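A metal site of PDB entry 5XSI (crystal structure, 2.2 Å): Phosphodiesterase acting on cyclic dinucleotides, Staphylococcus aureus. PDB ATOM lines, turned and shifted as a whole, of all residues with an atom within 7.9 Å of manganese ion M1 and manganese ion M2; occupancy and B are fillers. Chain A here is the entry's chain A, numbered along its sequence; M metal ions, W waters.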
ATOM      1  N   GLY A  30      19.904  32.304 -17.440  1.00  0.00           N
ATOM      2  CA  GLY A  30      20.713  31.450 -16.604  1.00  0.00           C
ATOM      3  C   GLY A  30      22.179  31.598 -16.909  1.00  0.00           C
ATOM      4  O   GLY A  30      22.644  32.649 -17.345  1.00  0.00           O
ATOM      5  N   HIS A  31      22.940  30.525 -16.689  1.00  0.00           N
ATOM      6  CA  HIS A  31      24.363  30.560 -16.871  1.00  0.00           C
ATOM      7  C   HIS A  31      24.746  30.048 -18.283  1.00  0.00           C
ATOM      8  O   HIS A  31      23.907  29.587 -19.071  1.00  0.00           O
ATOM      9  CB  HIS A  31      25.036  29.764 -15.744  1.00  0.00           C
ATOM     10  CG  HIS A  31      24.584  28.347 -15.673  1.00  0.00           C
ATOM     11  ND1 HIS A  31      25.025  27.382 -16.548  1.00  0.00           N
ATOM     12  CD2 HIS A  31      23.702  27.735 -14.832  1.00  0.00           C
ATOM     13  CE1 HIS A  31      24.451  26.217 -16.249  1.00  0.00           C
ATOM     14  NE2 HIS A  31      23.646  26.410 -15.212  1.00  0.00           N
ATOM     15  N   LYS A  32      26.009  30.222 -18.637  1.00  0.00           N
ATOM     16  CA  LYS A  32      26.519  29.715 -19.910  1.00  0.00           C
ATOM     17  C   LYS A  32      26.471  28.188 -19.928  1.00  0.00           C
ATOM     18  O   LYS A  32      26.664  27.520 -18.899  1.00  0.00           O
ATOM     19  CB  LYS A  32      27.956  30.156 -20.133  1.00  0.00           C
ATOM     20  CG  LYS A  32      28.112  31.670 -20.095  1.00  0.00           C
ATOM     21  CD  LYS A  32      29.556  32.051 -19.889  1.00  0.00           C
ATOM     22  CE  LYS A  32      29.975  33.156 -20.835  1.00  0.00           C
ATOM     23  NZ  LYS A  32      29.123  34.391 -20.828  1.00  0.00           N
ATOM     24  N   ARG A  33      26.162  27.660 -21.089  1.00  0.00           N
ATOM     25  CA  ARG A  33      25.993  26.240 -21.285  1.00  0.00           C
ATOM     26  C   ARG A  33      24.939  25.674 -20.345  1.00  0.00           C
ATOM     27  O   ARG A  33      25.240  24.902 -19.471  1.00  0.00           O
ATOM     28  CB  ARG A  33      27.328  25.558 -21.149  1.00  0.00           C
ATOM     29  CG  ARG A  33      27.781  24.960 -22.450  1.00  0.00           C
ATOM     30  CD  ARG A  33      26.608  24.259 -23.149  1.00  0.00           C
ATOM     31  NE  ARG A  33      27.058  23.497 -24.304  1.00  0.00           N
ATOM     32  CZ  ARG A  33      27.926  22.504 -24.257  1.00  0.00           C
ATOM     33  NH1 ARG A  33      28.421  22.120 -23.098  1.00  0.00           N
ATOM     34  NH2 ARG A  33      28.290  21.885 -25.350  1.00  0.00           N
ATOM     35  N   PRO A  34      23.710  26.088 -20.529  1.00  0.00           N
ATOM     36  CA  PRO A  34      22.732  25.926 -19.460  1.00  0.00           C
ATOM     37  C   PRO A  34      22.317  24.467 -19.321  1.00  0.00           C
ATOM     38  O   PRO A  34      22.196  23.743 -20.323  1.00  0.00           O
ATOM     39  CB  PRO A  34      21.585  26.834 -19.899  1.00  0.00           C
ATOM     40  CG  PRO A  34      21.785  26.937 -21.445  1.00  0.00           C
ATOM     41  CD  PRO A  34      23.228  26.950 -21.631  1.00  0.00           C
ATOM     42  N   ASP A  35      22.110  24.002 -18.109  1.00  0.00           N
ATOM     43  CA  ASP A  35      21.596  22.661 -17.877  1.00  0.00           C
ATOM     44  C   ASP A  35      20.085  22.725 -17.676  1.00  0.00           C
ATOM     45  O   ASP A  35      19.526  23.779 -17.840  1.00  0.00           O
ATOM     46  CB  ASP A  35      22.299  22.008 -16.718  1.00  0.00           C
ATOM     47  CG  ASP A  35      22.272  22.845 -15.498  1.00  0.00           C
ATOM     48  OD1 ASP A  35      21.329  23.547 -15.258  1.00  0.00           O
ATOM     49  OD2 ASP A  35      23.211  22.817 -14.761  1.00  0.00           O
ATOM     50  N   LEU A  36      19.443  21.610 -17.342  1.00  0.00           N
ATOM     51  CA  LEU A  36      17.985  21.588 -17.282  1.00  0.00           C
ATOM     52  C   LEU A  36      17.478  22.375 -16.067  1.00  0.00           C
ATOM     53  O   LEU A  36      16.382  22.902 -16.120  1.00  0.00           O
ATOM     54  CB  LEU A  36      17.434  20.125 -17.285  1.00  0.00           C
ATOM     55  CG  LEU A  36      17.661  19.440 -18.640  1.00  0.00           C
ATOM     56  CD1 LEU A  36      16.836  18.190 -18.859  1.00  0.00           C
ATOM     57  CD2 LEU A  36      17.390  20.366 -19.816  1.00  0.00           C
ATOM     58  N   ASP A  37      18.238  22.503 -14.997  1.00  0.00           N
ATOM     59  CA  ASP A  37      17.763  23.334 -13.865  1.00  0.00           C
ATOM     60  C   ASP A  37      17.749  24.827 -14.237  1.00  0.00           C
ATOM     61  O   ASP A  37      16.794  25.540 -13.954  1.00  0.00           O
ATOM     62  CB  ASP A  37      18.623  23.114 -12.621  1.00  0.00           C
ATOM     63  CG  ASP A  37      18.054  23.834 -11.404  1.00  0.00           C
ATOM     64  OD1 ASP A  37      16.835  23.811 -11.229  1.00  0.00           O
ATOM     65  OD2 ASP A  37      18.828  24.431 -10.622  1.00  0.00           O
ATOM     66  N   ALA A  38      18.794  25.288 -14.922  1.00  0.00           N
ATOM     67  CA  ALA A  38      18.789  26.651 -15.447  1.00  0.00           C
ATOM     68  C   ALA A  38      17.597  26.882 -16.402  1.00  0.00           C
ATOM     69  O   ALA A  38      16.928  27.906 -16.328  1.00  0.00           O
ATOM     70  CB  ALA A  38      20.128  26.942 -16.130  1.00  0.00           C
ATOM     71  N   ILE A  39      17.360  25.949 -17.322  1.00  0.00           N
ATOM     72  CA  ILE A  39      16.289  26.192 -18.288  1.00  0.00           C
ATOM     73  C   ILE A  39      14.916  26.041 -17.608  1.00  0.00           C
ATOM     74  O   ILE A  39      13.999  26.846 -17.812  1.00  0.00           O
ATOM     75  CB  ILE A  39      16.432  25.235 -19.490  1.00  0.00           C
ATOM     76  CG1 ILE A  39      17.678  25.573 -20.295  1.00  0.00           C
ATOM     77  CG2 ILE A  39      15.221  25.330 -20.376  1.00  0.00           C
ATOM     78  CD1 ILE A  39      17.648  27.025 -20.871  1.00  0.00           C
ATOM     79  N   ALA A  41      14.171  26.442 -14.337  1.00  0.00           N
ATOM     80  CA  ALA A  41      13.972  27.626 -13.502  1.00  0.00           C
ATOM     81  C   ALA A  41      13.574  28.840 -14.351  1.00  0.00           C
ATOM     82  O   ALA A  41      12.671  29.600 -13.979  1.00  0.00           O
ATOM     83  CB  ALA A  41      15.247  27.899 -12.667  1.00  0.00           C
ATOM     84  N   VAL A 105      18.853  33.364 -13.149  1.00  0.00           N
ATOM     85  CA  VAL A 105      18.476  32.114 -12.468  1.00  0.00           C
ATOM     86  C   VAL A 105      19.665  31.161 -12.453  1.00  0.00           C
ATOM     87  O   VAL A 105      20.363  31.010 -13.468  1.00  0.00           O
ATOM     88  CB  VAL A 105      17.231  31.419 -13.070  1.00  0.00           C
ATOM     89  CG1 VAL A 105      15.966  32.318 -12.898  1.00  0.00           C
ATOM     90  CG2 VAL A 105      17.420  31.050 -14.611  1.00  0.00           C
ATOM     91  N   ASP A 106      19.874  30.516 -11.297  1.00  0.00           N
ATOM     92  CA  ASP A 106      20.745  29.352 -11.162  1.00  0.00           C
ATOM     93  C   ASP A 106      22.235  29.683 -11.298  1.00  0.00           C
ATOM     94  O   ASP A 106      23.070  28.797 -11.541  1.00  0.00           O
ATOM     95  CB  ASP A 106      20.362  28.299 -12.210  1.00  0.00           C
ATOM     96  CG  ASP A 106      20.860  26.918 -11.818  1.00  0.00           C
ATOM     97  OD1 ASP A 106      20.907  26.637 -10.599  1.00  0.00           O
ATOM     98  OD2 ASP A 106      21.266  26.176 -12.724  1.00  0.00           O
ATOM     99  N   THR A 107      22.571  30.964 -11.190  1.00  0.00           N
ATOM    100  CA  THR A 107      23.941  31.381 -11.041  1.00  0.00           C
ATOM    101  C   THR A 107      23.842  32.752 -10.377  1.00  0.00           C
ATOM    102  O   THR A 107      22.756  33.326 -10.310  1.00  0.00           O
ATOM    103  CB  THR A 107      24.654  31.412 -12.398  1.00  0.00           C
ATOM    104  OG1 THR A 107      26.038  31.615 -12.215  1.00  0.00           O
ATOM    105  CG2 THR A 107      24.087  32.483 -13.243  1.00  0.00           C
ATOM    106  N   ASP A 129      19.051  31.736  -6.855  1.00  0.00           N
ATOM    107  CA  ASP A 129      20.111  30.732  -6.955  1.00  0.00           C
ATOM    108  C   ASP A 129      20.135  29.875  -5.703  1.00  0.00           C
ATOM    109  O   ASP A 129      19.681  30.292  -4.646  1.00  0.00           O
ATOM    110  CB  ASP A 129      21.466  31.417  -7.186  1.00  0.00           C
ATOM    111  CG  ASP A 129      22.558  30.443  -7.579  1.00  0.00           C
ATOM    112  OD1 ASP A 129      22.263  29.353  -8.109  1.00  0.00           O
ATOM    113  OD2 ASP A 129      23.726  30.781  -7.355  1.00  0.00           O
ATOM    114  N   HIS A 130      20.711  28.686  -5.817  1.00  0.00           N
ATOM    115  CA  HIS A 130      20.792  27.768  -4.672  1.00  0.00           C
ATOM    116  C   HIS A 130      22.241  27.429  -4.349  1.00  0.00           C
ATOM    117  O   HIS A 130      22.510  26.416  -3.677  1.00  0.00           O
ATOM    118  CB  HIS A 130      19.983  26.489  -4.957  1.00  0.00           C
ATOM    119  CG  HIS A 130      20.538  25.673  -6.099  1.00  0.00           C
ATOM    120  ND1 HIS A 130      21.214  24.474  -5.898  1.00  0.00           N
ATOM    121  CD2 HIS A 130      20.507  25.869  -7.441  1.00  0.00           C
ATOM    122  CE1 HIS A 130      21.580  23.989  -7.073  1.00  0.00           C
ATOM    123  NE2 HIS A 130      21.149  24.803  -8.022  1.00  0.00           N
ATOM    124  N   HIS A 131      23.205  28.149  -4.935  1.00  0.00           N
ATOM    125  CA  HIS A 131      24.605  27.859  -4.674  1.00  0.00           C
ATOM    126  C   HIS A 131      25.101  28.744  -3.518  1.00  0.00           C
ATOM    127  O   HIS A 131      24.430  29.705  -3.093  1.00  0.00           O
ATOM    128  CB  HIS A 131      25.446  28.045  -5.935  1.00  0.00           C
ATOM    129  CG  HIS A 131      25.007  27.191  -7.092  1.00  0.00           C
ATOM    130  ND1 HIS A 131      24.169  27.656  -8.100  1.00  0.00           N
ATOM    131  CD2 HIS A 131      25.299  25.907  -7.421  1.00  0.00           C
ATOM    132  CE1 HIS A 131      23.944  26.687  -8.975  1.00  0.00           C
ATOM    133  NE2 HIS A 131      24.641  25.628  -8.609  1.00  0.00           N
ATOM    134  N   ALA A 150      18.587  24.462  -0.662  1.00  0.00           N
ATOM    135  CA  ALA A 150      17.580  23.959  -1.606  1.00  0.00           C
ATOM    136  C   ALA A 150      18.209  23.020  -2.633  1.00  0.00           C
ATOM    137  O   ALA A 150      19.409  23.111  -2.920  1.00  0.00           O
ATOM    138  CB  ALA A 150      16.900  25.119  -2.352  1.00  0.00           C
ATOM    139  N   SER A 151      17.410  22.116  -3.195  1.00  0.00           N
ATOM    140  CA  SER A 151      17.965  21.197  -4.214  1.00  0.00           C
ATOM    141  C   SER A 151      18.434  21.898  -5.487  1.00  0.00           C
ATOM    142  O   SER A 151      19.294  21.369  -6.200  1.00  0.00           O
ATOM    143  CB  SER A 151      16.930  20.140  -4.660  1.00  0.00           C
ATOM    144  OG  SER A 151      15.812  20.706  -5.337  1.00  0.00           O
ATOM    145  N   SER A 152      17.803  23.011  -5.870  1.00  0.00           N
ATOM    146  CA  SER A 152      17.849  23.409  -7.270  1.00  0.00           C
ATOM    147  C   SER A 152      17.153  24.741  -7.388  1.00  0.00           C
ATOM    148  O   SER A 152      16.345  25.106  -6.505  1.00  0.00           O
ATOM    149  CB  SER A 152      17.150  22.364  -8.181  1.00  0.00           C
ATOM    150  OG  SER A 152      15.818  22.188  -7.708  1.00  0.00           O
ATOM    151  N   THR A 153      17.477  25.483  -8.450  1.00  0.00           N
ATOM    152  CA  THR A 153      16.717  26.702  -8.647  1.00  0.00           C
ATOM    153  C   THR A 153      15.282  26.373  -9.024  1.00  0.00           C
ATOM    154  O   THR A 153      14.366  27.131  -8.679  1.00  0.00           O
ATOM    155  CB  THR A 153      17.399  27.599  -9.709  1.00  0.00           C
ATOM    156  OG1 THR A 153      18.797  27.705  -9.406  1.00  0.00           O
ATOM    157  CG2 THR A 153      16.822  29.049  -9.716  1.00  0.00           C
ATOM    158  N   ALA A 154      15.057  25.226  -9.702  1.00  0.00           N
ATOM    159  CA  ALA A 154      13.682  24.814 -10.039  1.00  0.00           C
ATOM    160  C   ALA A 154      12.819  24.668  -8.788  1.00  0.00           C
ATOM    161  O   ALA A 154      11.645  25.094  -8.736  1.00  0.00           O
ATOM    162  CB  ALA A 154      13.700  23.500 -10.857  1.00  0.00           C
ATOM    163  N   GLY A 181      14.889  19.444 -14.152  1.00  0.00           N
ATOM    164  CA  GLY A 181      16.021  20.131 -13.528  1.00  0.00           C
ATOM    165  C   GLY A 181      16.185  19.738 -12.089  1.00  0.00           C
ATOM    166  O   GLY A 181      17.319  19.556 -11.604  1.00  0.00           O
ATOM    167  N   ILE A 182      15.066  19.489 -11.382  1.00  0.00           N
ATOM    168  CA  ILE A 182      15.195  18.844 -10.072  1.00  0.00           C
ATOM    169  C   ILE A 182      15.862  17.468 -10.185  1.00  0.00           C
ATOM    170  O   ILE A 182      16.793  17.160  -9.444  1.00  0.00           O
ATOM    171  CB  ILE A 182      13.845  18.772  -9.362  1.00  0.00           C
ATOM    172  CG1 ILE A 182      13.341  20.196  -9.175  1.00  0.00           C
ATOM    173  CG2 ILE A 182      13.976  18.002  -7.975  1.00  0.00           C
ATOM    174  CD1 ILE A 182      11.963  20.320  -8.460  1.00  0.00           C
ATOM    175  N   VAL A 184      17.949  16.227 -12.392  1.00  0.00           N
ATOM    176  CA  VAL A 184      19.400  16.339 -12.632  1.00  0.00           C
ATOM    177  C   VAL A 184      20.112  16.854 -11.378  1.00  0.00           C
ATOM    178  O   VAL A 184      21.029  16.215 -10.865  1.00  0.00           O
ATOM    179  CB  VAL A 184      19.698  17.214 -13.859  1.00  0.00           C
ATOM    180  CG1 VAL A 184      21.253  17.373 -14.038  1.00  0.00           C
ATOM    181  CG2 VAL A 184      19.121  16.575 -15.090  1.00  0.00           C
ATOM    182  N   ASP A 185      19.653  17.965 -10.823  1.00  0.00           N
ATOM    183  CA  ASP A 185      20.401  18.486  -9.684  1.00  0.00           C
ATOM    184  C   ASP A 185      20.417  17.550  -8.473  1.00  0.00           C
ATOM    185  O   ASP A 185      21.366  17.609  -7.700  1.00  0.00           O
ATOM    186  CB  ASP A 185      19.869  19.848  -9.297  1.00  0.00           C
ATOM    187  CG  ASP A 185      20.549  20.972 -10.088  1.00  0.00           C
ATOM    188  OD1 ASP A 185      21.151  20.687 -11.157  1.00  0.00           O
ATOM    189  OD2 ASP A 185      20.455  22.116  -9.642  1.00  0.00           O
ATOM    190  N   ARG A 192      20.896  16.287  -1.844  1.00  0.00           N
ATOM    191  CA  ARG A 192      20.304  17.557  -1.472  1.00  0.00           C
ATOM    192  C   ARG A 192      18.787  17.595  -1.604  1.00  0.00           C
ATOM    193  O   ARG A 192      18.254  18.515  -2.110  1.00  0.00           O
ATOM    194  CB  ARG A 192      20.962  18.676  -2.263  1.00  0.00           C
ATOM    195  CG  ARG A 192      22.441  18.848  -2.024  1.00  0.00           C
ATOM    196  CD  ARG A 192      22.981  20.198  -2.440  1.00  0.00           C
ATOM    197  NE  ARG A 192      22.420  20.631  -3.705  1.00  0.00           N
ATOM    198  CZ  ARG A 192      22.431  19.893  -4.799  1.00  0.00           C
ATOM    199  NH1 ARG A 192      22.992  18.720  -4.759  1.00  0.00           N
ATOM    200  NH2 ARG A 192      21.922  20.351  -5.917  1.00  0.00           N
HETATM  201 MN    MN M   1      23.013  24.700 -13.228  1.00  0.00          MN
HETATM  202 MN    MN M   2      21.036  24.247 -10.296  1.00  0.00          MN
HETATM  203  O   HOH W   1      22.191  23.123 -11.770  1.00  0.00           O
HETATM  204  O   HOH W   2      23.657  23.597  -9.871  1.00  0.00           O
HETATM  205  O   HOH W   3      25.128  26.117 -12.031  1.00  0.00           O
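Water W3 lies within hydrogen-bond range of O of Asp 106 (3.4 Å) and NE2 of His 131 (3.5 Å).
Manganese ion M1 is bound by water W1 (2.3 Å), the side-chain carboxylate of Asp 106 (2.3 Å), the side-chain carboxylate of Asp 35 (2.4 Å) and a ring nitrogen (NE2) of His 31 (2.7 Å).
Manganese ion M1 has four donor atoms within binding distance.
Slightly farther from manganese ion M1 lies water W3 (2.8 Å).
Slightly farther from manganese ion M1 lies the side-chain carboxylate (OD1) of Asp 35 (2.9 Å).
N of Asp 37 lies close to OD1 of Asp 35, at 3.3 Å.
The side-chain carboxylate (OD1) of Asp 37 sits at hydrogen-bond distance from the backbone NH (N) of Thr 153, 3.3 Å away.
The side-chain carboxylate of Asp 37 lies within hydrogen-bond range of the backbone NH of Ala 154 (2.7 Å).
The backbone carbonyl oxygen of Asp 185 sits at hydrogen-bond distance from the guanidinium group of Arg 192, at 3.3 Å.
OD1 of Asp 106 sits close to OG1 of Thr 153, at 2.6 Å.
The side-chain carboxylate (OD2) of Asp 106 lies close to the backbone NH (N) of Ala 38 (3.4 Å).
The side-chain carboxylate of Asp 35 lies within hydrogen-bond range of the backbone NH of Ala 38, 3.1 Å away.
Manganese ion M2 is bound by water W1 (2.2 Å), OD2 of Asp 37 (2.2 Å), OD2 of Asp 185 (2.3 Å), NE2 of His 130 (2.3 Å) and OD1 of Asp 106 (2.4 Å).
Slightly farther from manganese ion M2 lies water W2 (2.7 Å).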
